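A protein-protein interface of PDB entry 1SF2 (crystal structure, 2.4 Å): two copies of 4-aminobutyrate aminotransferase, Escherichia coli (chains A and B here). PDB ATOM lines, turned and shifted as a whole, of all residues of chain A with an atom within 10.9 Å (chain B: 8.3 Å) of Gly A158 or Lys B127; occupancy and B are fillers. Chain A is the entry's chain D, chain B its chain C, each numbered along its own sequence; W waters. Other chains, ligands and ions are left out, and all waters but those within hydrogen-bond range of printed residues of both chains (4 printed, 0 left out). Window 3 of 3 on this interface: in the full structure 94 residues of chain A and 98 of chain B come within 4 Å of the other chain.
The backbone carbonyl oxygen of Arg B123 sits at hydrogen-bond distance from the backbone NH of Arg B128 (3.4 Å). NH2 of Arg B123 lies within hydrogen-bond range of OG of Ser B129, at 3.2 Å. N of Arg B128 lies close to OG1 of Thr B126. O of Glu B198 lies close to NE of Arg B128 (3.5 Å). The backbone carbonyl oxygen (O) of Ile B200 is in hydrogen-bond range of the guanidinium group (NH1) of Arg B128, 3.0 Å away. The guanidinium group of Arg B128 sits at hydrogen-bond distance from the backbone carbonyl oxygen of Gly B233.
Water W1 lies within hydrogen-bond range of the backbone carbonyl oxygen of Ala A157 (2.5 Å), the backbone NH of Ala B290 (3.0 Å) and the backbone carbonyl oxygen of Pro A154 (3.3 Å). Water W2 lies within hydrogen-bond range of the side-chain amino group (NZ) of Lys B120 (2.6 Å) and the backbone carbonyl oxygen (O) of Tyr A155 (3.1 Å). Water W3 lies within hydrogen-bond range of the guanidinium group of Arg B123 (3.0 Å) and the backbone carbonyl oxygen of Leu A161 (3.1 Å). Water W4 lies within hydrogen-bond range of N of Leu A161 and OG of Ser B129.
Gly A158 touches three residues of chain B. Printed residues of chain A within 4 Å of Lys B127: Gly A158. No residue of chain B comes within 4 Å of Ala A157. Of the printed residues of chain A, Ala B124 touches Gly A158. No residue of chain A comes within 4 Å of Thr B126. Printed residues of chain A within 4 Å of Lys B120: His A143 (3.8 Å), Leu A146 (3.8 Å) and Met A159 (3.6 Å). Of the printed residues of chain A, Ser B129 touches Met A159 (3.6 Å). Ala B201 touches none of the printed residues of chain A. The nearest residue of chain A that does not touch Lys B127 is Met A159 (5.5 Å). The nearest printed residue of chain B that does not touch Met A159 is Val B289 (4.03 Å).
His A143 touches Lys B120 (CE1 to CG, 3.8 Å). Leu A146 touches Lys B120 (CD1 to CD, 3.8 Å). Gly A158 touches Ala B124 (O to CA, 3.7 Å). Gly A158 touches Lys B127 (O to CA, 3.9 Å). Met A159 touches Lys B120 (CG to O, 3.6 Å). O of Met A159 touches O of Arg B128 (3.6 Å). Met A159 touches Ser B129 (O to OG, 3.6 Å). NH2 of Arg B123 touches C of Gly A160 (3.7 Å). Arg B123 touches Met A162 (NH2 to CE, 3.9 Å).
NH1 of Arg B123 is in hydrogen-bond range of NE2 of His A143, at 3.3 Å. O of Met A159 sits at hydrogen-bond distance from NH2 of Arg B123 (2.9 Å). The backbone carbonyl oxygen of Leu A161 is in hydrogen-bond range of the guanidinium group of Arg B123 (3.1 Å). The backbone carbonyl oxygen of Ala B288 is in hydrogen-bond range of the guanidinium group of Arg A17 (3.4 Å). The guanidinium group of Arg A17 lies within hydrogen-bond range of the backbone carbonyl oxygen of Val B289, 3.4 Å away. The backbone carbonyl oxygen (O) of Gly A158 sits close to the backbone carbonyl oxygen (O) of Arg B123, 3.3 Å away.
No position is printed for both chains.
Of the 14 printed residues of chain A, 8 touch a printed residue of chain B. Hydrophobic or aromatic side chains of chain A within 4 Å of the printed part of chain B: His A143, Leu A146, Met A159 and Met A162. Printed residues of chain B that touch a printed residue of chain A: Lys B120, Arg B123, Ala B124, Lys B127, Arg B128, Ser B129, Ala B288 and Val B289.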
ATOM      1  N   ARG A  17       2.857 -27.736 -11.867  1.00  0.00           N
ATOM      2  CA  ARG A  17       2.877 -28.925 -11.032  1.00  0.00           C
ATOM      3  C   ARG A  17       1.562 -29.095 -10.276  1.00  0.00           C
ATOM      4  O   ARG A  17       1.265 -30.183  -9.770  1.00  0.00           O
ATOM      5  CB  ARG A  17       4.037 -28.848 -10.041  1.00  0.00           C
ATOM      6  CG  ARG A  17       4.088 -27.547  -9.274  1.00  0.00           C
ATOM      7  CD  ARG A  17       5.014 -27.623  -8.068  1.00  0.00           C
ATOM      8  NE  ARG A  17       4.751 -26.491  -7.185  1.00  0.00           N
ATOM      9  CZ  ARG A  17       4.824 -26.529  -5.861  1.00  0.00           C
ATOM     10  NH1 ARG A  17       5.164 -27.656  -5.241  1.00  0.00           N
ATOM     11  NH2 ARG A  17       4.532 -25.440  -5.156  1.00  0.00           N
ATOM     12  N   HIS A 143     -14.026 -21.895  -5.781  1.00  0.00           N
ATOM     13  CA  HIS A 143     -13.879 -21.465  -4.399  1.00  0.00           C
ATOM     14  C   HIS A 143     -14.969 -22.037  -3.522  1.00  0.00           C
ATOM     15  O   HIS A 143     -14.687 -22.665  -2.496  1.00  0.00           O
ATOM     16  CB  HIS A 143     -13.914 -19.939  -4.268  1.00  0.00           C
ATOM     17  CG  HIS A 143     -12.619 -19.265  -4.608  1.00  0.00           C
ATOM     18  ND1 HIS A 143     -12.168 -19.117  -5.904  1.00  0.00           N
ATOM     19  CD2 HIS A 143     -11.692 -18.668  -3.819  1.00  0.00           C
ATOM     20  CE1 HIS A 143     -11.024 -18.455  -5.898  1.00  0.00           C
ATOM     21  NE2 HIS A 143     -10.713 -18.171  -4.646  1.00  0.00           N
ATOM     22  N   LEU A 146     -14.994 -25.764  -3.165  1.00  0.00           N
ATOM     23  CA  LEU A 146     -13.834 -26.191  -2.380  1.00  0.00           C
ATOM     24  C   LEU A 146     -14.235 -26.072  -0.899  1.00  0.00           C
ATOM     25  O   LEU A 146     -13.807 -26.878  -0.061  1.00  0.00           O
ATOM     26  CB  LEU A 146     -12.606 -25.318  -2.659  1.00  0.00           C
ATOM     27  CG  LEU A 146     -11.742 -25.740  -3.852  1.00  0.00           C
ATOM     28  CD1 LEU A 146     -10.554 -24.810  -3.970  1.00  0.00           C
ATOM     29  CD2 LEU A 146     -11.270 -27.169  -3.667  1.00  0.00           C
ATOM     30  N   VAL A 152      -9.005 -30.080   2.814  1.00  0.00           N
ATOM     31  CA  VAL A 152      -8.307 -28.836   2.515  1.00  0.00           C
ATOM     32  C   VAL A 152      -7.054 -28.982   1.655  1.00  0.00           C
ATOM     33  O   VAL A 152      -6.870 -28.243   0.691  1.00  0.00           O
ATOM     34  CB  VAL A 152      -7.922 -28.108   3.806  1.00  0.00           C
ATOM     35  CG1 VAL A 152      -7.180 -26.816   3.467  1.00  0.00           C
ATOM     36  CG2 VAL A 152      -9.172 -27.833   4.625  1.00  0.00           C
ATOM     37  N   ASN A 153      -6.196 -29.933   2.017  1.00  0.00           N
ATOM     38  CA  ASN A 153      -4.941 -30.190   1.312  1.00  0.00           C
ATOM     39  C   ASN A 153      -5.149 -31.210   0.201  1.00  0.00           C
ATOM     40  O   ASN A 153      -5.771 -32.241   0.425  1.00  0.00           O
ATOM     41  CB  ASN A 153      -3.900 -30.725   2.306  1.00  0.00           C
ATOM     42  CG  ASN A 153      -2.653 -31.286   1.622  1.00  0.00           C
ATOM     43  OD1 ASN A 153      -1.822 -30.534   1.099  1.00  0.00           O
ATOM     44  ND2 ASN A 153      -2.524 -32.618   1.619  1.00  0.00           N
ATOM     45  N   PRO A 154      -4.593 -30.958  -1.002  1.00  0.00           N
ATOM     46  CA  PRO A 154      -3.782 -29.787  -1.369  1.00  0.00           C
ATOM     47  C   PRO A 154      -4.539 -28.691  -2.123  1.00  0.00           C
ATOM     48  O   PRO A 154      -3.940 -27.680  -2.519  1.00  0.00           O
ATOM     49  CB  PRO A 154      -2.700 -30.401  -2.237  1.00  0.00           C
ATOM     50  CG  PRO A 154      -3.515 -31.364  -3.063  1.00  0.00           C
ATOM     51  CD  PRO A 154      -4.491 -31.995  -2.047  1.00  0.00           C
ATOM     52  N   TYR A 155      -5.842 -28.890  -2.322  1.00  0.00           N
ATOM     53  CA  TYR A 155      -6.676 -27.921  -3.049  1.00  0.00           C
ATOM     54  C   TYR A 155      -6.532 -26.450  -2.607  1.00  0.00           C
ATOM     55  O   TYR A 155      -6.338 -25.553  -3.448  1.00  0.00           O
ATOM     56  CB  TYR A 155      -8.147 -28.319  -2.940  1.00  0.00           C
ATOM     57  CG  TYR A 155      -8.439 -29.787  -3.185  1.00  0.00           C
ATOM     58  CD1 TYR A 155      -9.537 -30.400  -2.582  1.00  0.00           C
ATOM     59  CD2 TYR A 155      -7.639 -30.564  -4.031  1.00  0.00           C
ATOM     60  CE1 TYR A 155      -9.837 -31.753  -2.802  1.00  0.00           C
ATOM     61  CE2 TYR A 155      -7.939 -31.933  -4.270  1.00  0.00           C
ATOM     62  CZ  TYR A 155      -9.039 -32.513  -3.644  1.00  0.00           C
ATOM     63  OH  TYR A 155      -9.339 -33.847  -3.827  1.00  0.00           O
ATOM     64  N   SER A 156      -6.608 -26.210  -1.297  1.00  0.00           N
ATOM     65  CA  SER A 156      -6.550 -24.856  -0.745  1.00  0.00           C
ATOM     66  C   SER A 156      -5.175 -24.413  -0.255  1.00  0.00           C
ATOM     67  O   SER A 156      -4.992 -23.253   0.147  1.00  0.00           O
ATOM     68  CB  SER A 156      -7.562 -24.741   0.412  1.00  0.00           C
ATOM     69  OG  SER A 156      -8.794 -25.410   0.106  1.00  0.00           O
ATOM     70  N   ALA A 157      -4.206 -25.323  -0.295  1.00  0.00           N
ATOM     71  CA  ALA A 157      -2.863 -25.026   0.188  1.00  0.00           C
ATOM     72  C   ALA A 157      -2.291 -23.679  -0.242  1.00  0.00           C
ATOM     73  O   ALA A 157      -2.208 -23.372  -1.425  1.00  0.00           O
ATOM     74  CB  ALA A 157      -1.923 -26.135  -0.221  1.00  0.00           C
ATOM     75  N   GLY A 158      -1.892 -22.876   0.736  1.00  0.00           N
ATOM     76  CA  GLY A 158      -1.300 -21.582   0.454  1.00  0.00           C
ATOM     77  C   GLY A 158      -2.254 -20.487   0.021  1.00  0.00           C
ATOM     78  O   GLY A 158      -1.893 -19.302   0.032  1.00  0.00           O
ATOM     79  N   MET A 159      -3.472 -20.869  -0.354  1.00  0.00           N
ATOM     80  CA  MET A 159      -4.466 -19.908  -0.820  1.00  0.00           C
ATOM     81  C   MET A 159      -5.137 -19.123   0.294  1.00  0.00           C
ATOM     82  O   MET A 159      -5.513 -17.959   0.117  1.00  0.00           O
ATOM     83  CB  MET A 159      -5.527 -20.634  -1.634  1.00  0.00           C
ATOM     84  CG  MET A 159      -4.977 -21.319  -2.858  1.00  0.00           C
ATOM     85  SD  MET A 159      -6.152 -22.443  -3.569  1.00  0.00           S
ATOM     86  CE  MET A 159      -5.194 -23.166  -4.892  1.00  0.00           C
ATOM     87  N   GLY A 160      -5.276 -19.755   1.452  1.00  0.00           N
ATOM     88  CA  GLY A 160      -5.937 -19.103   2.563  1.00  0.00           C
ATOM     89  C   GLY A 160      -7.284 -19.780   2.720  1.00  0.00           C
ATOM     90  O   GLY A 160      -7.536 -20.795   2.065  1.00  0.00           O
ATOM     91  N   LEU A 161      -8.149 -19.224   3.565  1.00  0.00           N
ATOM     92  CA  LEU A 161      -9.467 -19.795   3.806  1.00  0.00           C
ATOM     93  C   LEU A 161     -10.455 -19.579   2.657  1.00  0.00           C
ATOM     94  O   LEU A 161     -10.541 -18.489   2.092  1.00  0.00           O
ATOM     95  CB  LEU A 161     -10.047 -19.226   5.104  1.00  0.00           C
ATOM     96  CG  LEU A 161      -9.246 -19.655   6.341  1.00  0.00           C
ATOM     97  CD1 LEU A 161      -9.709 -18.879   7.545  1.00  0.00           C
ATOM     98  CD2 LEU A 161      -9.379 -21.178   6.563  1.00  0.00           C
ATOM     99  N   MET A 162     -11.183 -20.637   2.307  1.00  0.00           N
ATOM    100  CA  MET A 162     -12.192 -20.580   1.254  1.00  0.00           C
ATOM    101  C   MET A 162     -13.450 -19.901   1.825  1.00  0.00           C
ATOM    102  O   MET A 162     -13.521 -19.637   3.014  1.00  0.00           O
ATOM    103  CB  MET A 162     -12.518 -21.995   0.787  1.00  0.00           C
ATOM    104  CG  MET A 162     -11.421 -22.647  -0.032  1.00  0.00           C
ATOM    105  SD  MET A 162     -11.057 -21.729  -1.536  1.00  0.00           S
ATOM    106  CE  MET A 162      -9.617 -20.818  -1.062  1.00  0.00           C
ATOM    107  N   LYS B 120      -7.210 -18.546  -7.654  1.00  0.00           N
ATOM    108  CA  LYS B 120      -6.645 -19.516  -6.727  1.00  0.00           C
ATOM    109  C   LYS B 120      -5.121 -19.499  -6.877  1.00  0.00           C
ATOM    110  O   LYS B 120      -4.379 -19.483  -5.880  1.00  0.00           O
ATOM    111  CB  LYS B 120      -7.143 -20.931  -7.017  1.00  0.00           C
ATOM    112  CG  LYS B 120      -8.593 -21.205  -6.675  1.00  0.00           C
ATOM    113  CD  LYS B 120      -8.892 -22.708  -6.669  1.00  0.00           C
ATOM    114  CE  LYS B 120      -8.641 -23.377  -8.009  1.00  0.00           C
ATOM    115  NZ  LYS B 120      -9.009 -24.825  -7.960  1.00  0.00           N
ATOM    116  N   ILE B 121      -4.663 -19.486  -8.127  1.00  0.00           N
ATOM    117  CA  ILE B 121      -3.240 -19.477  -8.418  1.00  0.00           C
ATOM    118  C   ILE B 121      -2.564 -18.233  -7.851  1.00  0.00           C
ATOM    119  O   ILE B 121      -1.511 -18.322  -7.226  1.00  0.00           O
ATOM    120  CB  ILE B 121      -3.000 -19.556  -9.942  1.00  0.00           C
ATOM    121  CG1 ILE B 121      -3.398 -20.960 -10.450  1.00  0.00           C
ATOM    122  CG2 ILE B 121      -1.533 -19.210 -10.263  1.00  0.00           C
ATOM    123  CD1 ILE B 121      -3.360 -21.110 -11.976  1.00  0.00           C
ATOM    124  N   ALA B 122      -3.182 -17.076  -8.068  1.00  0.00           N
ATOM    125  CA  ALA B 122      -2.637 -15.812  -7.582  1.00  0.00           C
ATOM    126  C   ALA B 122      -2.537 -15.806  -6.060  1.00  0.00           C
ATOM    127  O   ALA B 122      -1.568 -15.288  -5.505  1.00  0.00           O
ATOM    128  CB  ALA B 122      -3.507 -14.642  -8.059  1.00  0.00           C
ATOM    129  N   ARG B 123      -3.537 -16.388  -5.392  1.00  0.00           N
ATOM    130  CA  ARG B 123      -3.563 -16.447  -3.927  1.00  0.00           C
ATOM    131  C   ARG B 123      -2.457 -17.343  -3.366  1.00  0.00           C
ATOM    132  O   ARG B 123      -1.822 -17.008  -2.358  1.00  0.00           O
ATOM    133  CB  ARG B 123      -4.936 -16.925  -3.444  1.00  0.00           C
ATOM    134  CG  ARG B 123      -6.067 -15.936  -3.739  1.00  0.00           C
ATOM    135  CD  ARG B 123      -7.422 -16.421  -3.252  1.00  0.00           C
ATOM    136  NE  ARG B 123      -7.404 -16.785  -1.839  1.00  0.00           N
ATOM    137  CZ  ARG B 123      -8.492 -17.052  -1.121  1.00  0.00           C
ATOM    138  NH1 ARG B 123      -9.689 -16.994  -1.697  1.00  0.00           N
ATOM    139  NH2 ARG B 123      -8.385 -17.360   0.171  1.00  0.00           N
ATOM    140  N   ALA B 124      -2.230 -18.484  -4.009  1.00  0.00           N
ATOM    141  CA  ALA B 124      -1.170 -19.389  -3.569  1.00  0.00           C
ATOM    142  C   ALA B 124       0.193 -18.713  -3.800  1.00  0.00           C
ATOM    143  O   ALA B 124       1.120 -18.875  -3.016  1.00  0.00           O
ATOM    144  CB  ALA B 124      -1.240 -20.714  -4.349  1.00  0.00           C
ATOM    145  N   ALA B 125       0.287 -17.947  -4.880  1.00  0.00           N
ATOM    146  CA  ALA B 125       1.505 -17.241  -5.259  1.00  0.00           C
ATOM    147  C   ALA B 125       1.874 -16.064  -4.368  1.00  0.00           C
ATOM    148  O   ALA B 125       3.054 -15.763  -4.179  1.00  0.00           O
ATOM    149  CB  ALA B 125       1.381 -16.756  -6.701  1.00  0.00           C
ATOM    150  N   THR B 126       0.877 -15.382  -3.823  1.00  0.00           N
ATOM    151  CA  THR B 126       1.167 -14.224  -2.994  1.00  0.00           C
ATOM    152  C   THR B 126       0.902 -14.461  -1.530  1.00  0.00           C
ATOM    153  O   THR B 126       1.312 -13.652  -0.687  1.00  0.00           O
ATOM    154  CB  THR B 126       0.324 -12.998  -3.407  1.00  0.00           C
ATOM    155  OG1 THR B 126      -1.065 -13.265  -3.147  1.00  0.00           O
ATOM    156  CG2 THR B 126       0.518 -12.681  -4.875  1.00  0.00           C
ATOM    157  N   LYS B 127       0.206 -15.547  -1.214  1.00  0.00           N
ATOM    158  CA  LYS B 127      -0.124 -15.819   0.183  1.00  0.00           C
ATOM    159  C   LYS B 127      -1.112 -14.754   0.673  1.00  0.00           C
ATOM    160  O   LYS B 127      -1.032 -14.301   1.811  1.00  0.00           O
ATOM    161  CB  LYS B 127       1.135 -15.770   1.058  1.00  0.00           C
ATOM    162  CG  LYS B 127       2.230 -16.757   0.681  1.00  0.00           C
ATOM    163  CD  LYS B 127       1.784 -18.165   0.932  1.00  0.00           C
ATOM    164  CE  LYS B 127       2.939 -19.138   0.815  1.00  0.00           C
ATOM    165  NZ  LYS B 127       2.480 -20.514   1.197  1.00  0.00           N
ATOM    166  N   ARG B 128      -2.040 -14.359  -0.192  1.00  0.00           N
ATOM    167  CA  ARG B 128      -3.029 -13.344   0.149  1.00  0.00           C
ATOM    168  C   ARG B 128      -4.416 -13.846  -0.242  1.00  0.00           C
ATOM    169  O   ARG B 128      -4.538 -14.725  -1.097  1.00  0.00           O
ATOM    170  CB  ARG B 128      -2.716 -12.042  -0.592  1.00  0.00           C
ATOM    171  CG  ARG B 128      -1.295 -11.541  -0.375  1.00  0.00           C
ATOM    172  CD  ARG B 128      -1.035 -10.265  -1.158  1.00  0.00           C
ATOM    173  NE  ARG B 128       0.341  -9.818  -0.979  1.00  0.00           N
ATOM    174  CZ  ARG B 128       0.916  -8.840  -1.675  1.00  0.00           C
ATOM    175  NH1 ARG B 128       0.236  -8.186  -2.614  1.00  0.00           N
ATOM    176  NH2 ARG B 128       2.185  -8.526  -1.435  1.00  0.00           N
ATOM    177  N   SER B 129      -5.456 -13.276   0.359  1.00  0.00           N
ATOM    178  CA  SER B 129      -6.817 -13.715   0.089  1.00  0.00           C
ATOM    179  C   SER B 129      -7.748 -12.770  -0.677  1.00  0.00           C
ATOM    180  O   SER B 129      -8.731 -13.227  -1.264  1.00  0.00           O
ATOM    181  CB  SER B 129      -7.483 -14.080   1.406  1.00  0.00           C
ATOM    182  OG  SER B 129      -6.824 -15.177   1.996  1.00  0.00           O
ATOM    183  N   GLY B 130      -7.456 -11.471  -0.674  1.00  0.00           N
ATOM    184  CA  GLY B 130      -8.334 -10.530  -1.340  1.00  0.00           C
ATOM    185  C   GLY B 130      -8.111 -10.288  -2.817  1.00  0.00           C
ATOM    186  O   GLY B 130      -7.030 -10.548  -3.357  1.00  0.00           O
ATOM    187  N   GLU B 198      -1.080  -5.638   0.956  1.00  0.00           N
ATOM    188  CA  GLU B 198      -0.563  -6.937   1.368  1.00  0.00           C
ATOM    189  C   GLU B 198      -1.620  -8.011   1.604  1.00  0.00           C
ATOM    190  O   GLU B 198      -1.300  -9.127   2.007  1.00  0.00           O
ATOM    191  CB  GLU B 198       0.329  -6.806   2.611  1.00  0.00           C
ATOM    192  CG  GLU B 198      -0.368  -6.384   3.889  1.00  0.00           C
ATOM    193  CD  GLU B 198      -0.359  -4.871   4.122  1.00  0.00           C
ATOM    194  OE1 GLU B 198      -0.585  -4.480   5.293  1.00  0.00           O
ATOM    195  OE2 GLU B 198      -0.138  -4.083   3.162  1.00  0.00           O
ATOM    196  N   ASP B 199      -2.878  -7.680   1.357  1.00  0.00           N
ATOM    197  CA  ASP B 199      -3.956  -8.641   1.519  1.00  0.00           C
ATOM    198  C   ASP B 199      -4.646  -8.800   0.179  1.00  0.00           C
ATOM    199  O   ASP B 199      -5.620  -9.528   0.067  1.00  0.00           O
ATOM    200  CB  ASP B 199      -4.960  -8.164   2.564  1.00  0.00           C
ATOM    201  CG  ASP B 199      -4.490  -8.421   3.981  1.00  0.00           C
ATOM    202  OD1 ASP B 199      -4.444  -7.458   4.782  1.00  0.00           O
ATOM    203  OD2 ASP B 199      -4.177  -9.591   4.298  1.00  0.00           O
ATOM    204  N   ILE B 200      -4.153  -8.091  -0.835  1.00  0.00           N
ATOM    205  CA  ILE B 200      -4.719  -8.190  -2.178  1.00  0.00           C
ATOM    206  C   ILE B 200      -3.811  -9.099  -3.009  1.00  0.00           C
ATOM    207  O   ILE B 200      -2.648  -8.788  -3.258  1.00  0.00           O
ATOM    208  CB  ILE B 200      -4.848  -6.800  -2.861  1.00  0.00           C
ATOM    209  CG1 ILE B 200      -5.830  -5.916  -2.078  1.00  0.00           C
ATOM    210  CG2 ILE B 200      -5.349  -6.959  -4.294  1.00  0.00           C
ATOM    211  CD1 ILE B 200      -7.215  -6.524  -1.896  1.00  0.00           C
ATOM    212  N   ALA B 201      -4.352 -10.242  -3.411  1.00  0.00           N
ATOM    213  CA  ALA B 201      -3.606 -11.215  -4.186  1.00  0.00           C
ATOM    214  C   ALA B 201      -3.586 -10.837  -5.660  1.00  0.00           C
ATOM    215  O   ALA B 201      -2.593 -11.059  -6.363  1.00  0.00           O
ATOM    216  CB  ALA B 201      -4.230 -12.616  -4.003  1.00  0.00           C
ATOM    217  N   GLY B 233       3.369  -6.151  -5.429  1.00  0.00           N
ATOM    218  CA  GLY B 233       3.413  -7.592  -5.551  1.00  0.00           C
ATOM    219  C   GLY B 233       2.047  -8.211  -5.745  1.00  0.00           C
ATOM    220  O   GLY B 233       1.794  -9.333  -5.310  1.00  0.00           O
ATOM    221  N   MET B 235      -0.864  -9.675  -8.260  1.00  0.00           N
ATOM    222  CA  MET B 235      -0.910 -10.336  -9.555  1.00  0.00           C
ATOM    223  C   MET B 235      -1.943  -9.654 -10.436  1.00  0.00           C
ATOM    224  O   MET B 235      -3.079  -9.449 -10.028  1.00  0.00           O
ATOM    225  CB  MET B 235      -1.270 -11.816  -9.388  1.00  0.00           C
ATOM    226  CG  MET B 235      -0.292 -12.615  -8.554  1.00  0.00           C
ATOM    227  SD  MET B 235       1.351 -12.738  -9.336  1.00  0.00           S
ATOM    228  CE  MET B 235       2.219 -11.366  -8.553  1.00  0.00           C
ATOM    229  N   ALA B 288       3.030 -21.902  -7.993  1.00  0.00           N
ATOM    230  CA  ALA B 288       2.773 -21.705  -6.567  1.00  0.00           C
ATOM    231  C   ALA B 288       1.838 -22.759  -5.985  1.00  0.00           C
ATOM    232  O   ALA B 288       2.007 -23.183  -4.847  1.00  0.00           O
ATOM    233  CB  ALA B 288       2.193 -20.316  -6.322  1.00  0.00           C
ATOM    234  N   VAL B 289       0.849 -23.179  -6.759  1.00  0.00           N
ATOM    235  CA  VAL B 289      -0.101 -24.149  -6.261  1.00  0.00           C
ATOM    236  C   VAL B 289       0.580 -25.491  -6.029  1.00  0.00           C
ATOM    237  O   VAL B 289       1.364 -25.960  -6.863  1.00  0.00           O
ATOM    238  CB  VAL B 289      -1.289 -24.304  -7.243  1.00  0.00           C
ATOM    239  CG1 VAL B 289      -2.311 -25.319  -6.703  1.00  0.00           C
ATOM    240  CG2 VAL B 289      -1.959 -22.959  -7.437  1.00  0.00           C
ATOM    241  N   ALA B 290       0.269 -26.103  -4.887  1.00  0.00           N
ATOM    242  CA  ALA B 290       0.840 -27.393  -4.511  1.00  0.00           C
ATOM    243  C   ALA B 290       0.398 -28.463  -5.477  1.00  0.00           C
ATOM    244  O   ALA B 290      -0.707 -28.413  -6.007  1.00  0.00           O
ATOM    245  CB  ALA B 290       0.413 -27.759  -3.105  1.00  0.00           C
HETATM  246  O   HOH W   1      -1.993 -25.103  -3.157  1.00  0.00           O
HETATM  247  O   HOH W   2      -7.899 -26.245  -6.035  1.00  0.00           O
HETATM  248  O   HOH W   3     -12.282 -17.428  -0.268  1.00  0.00           O
HETATM  249  O   HOH W   4      -7.793 -16.349   4.802  1.00  0.00           O
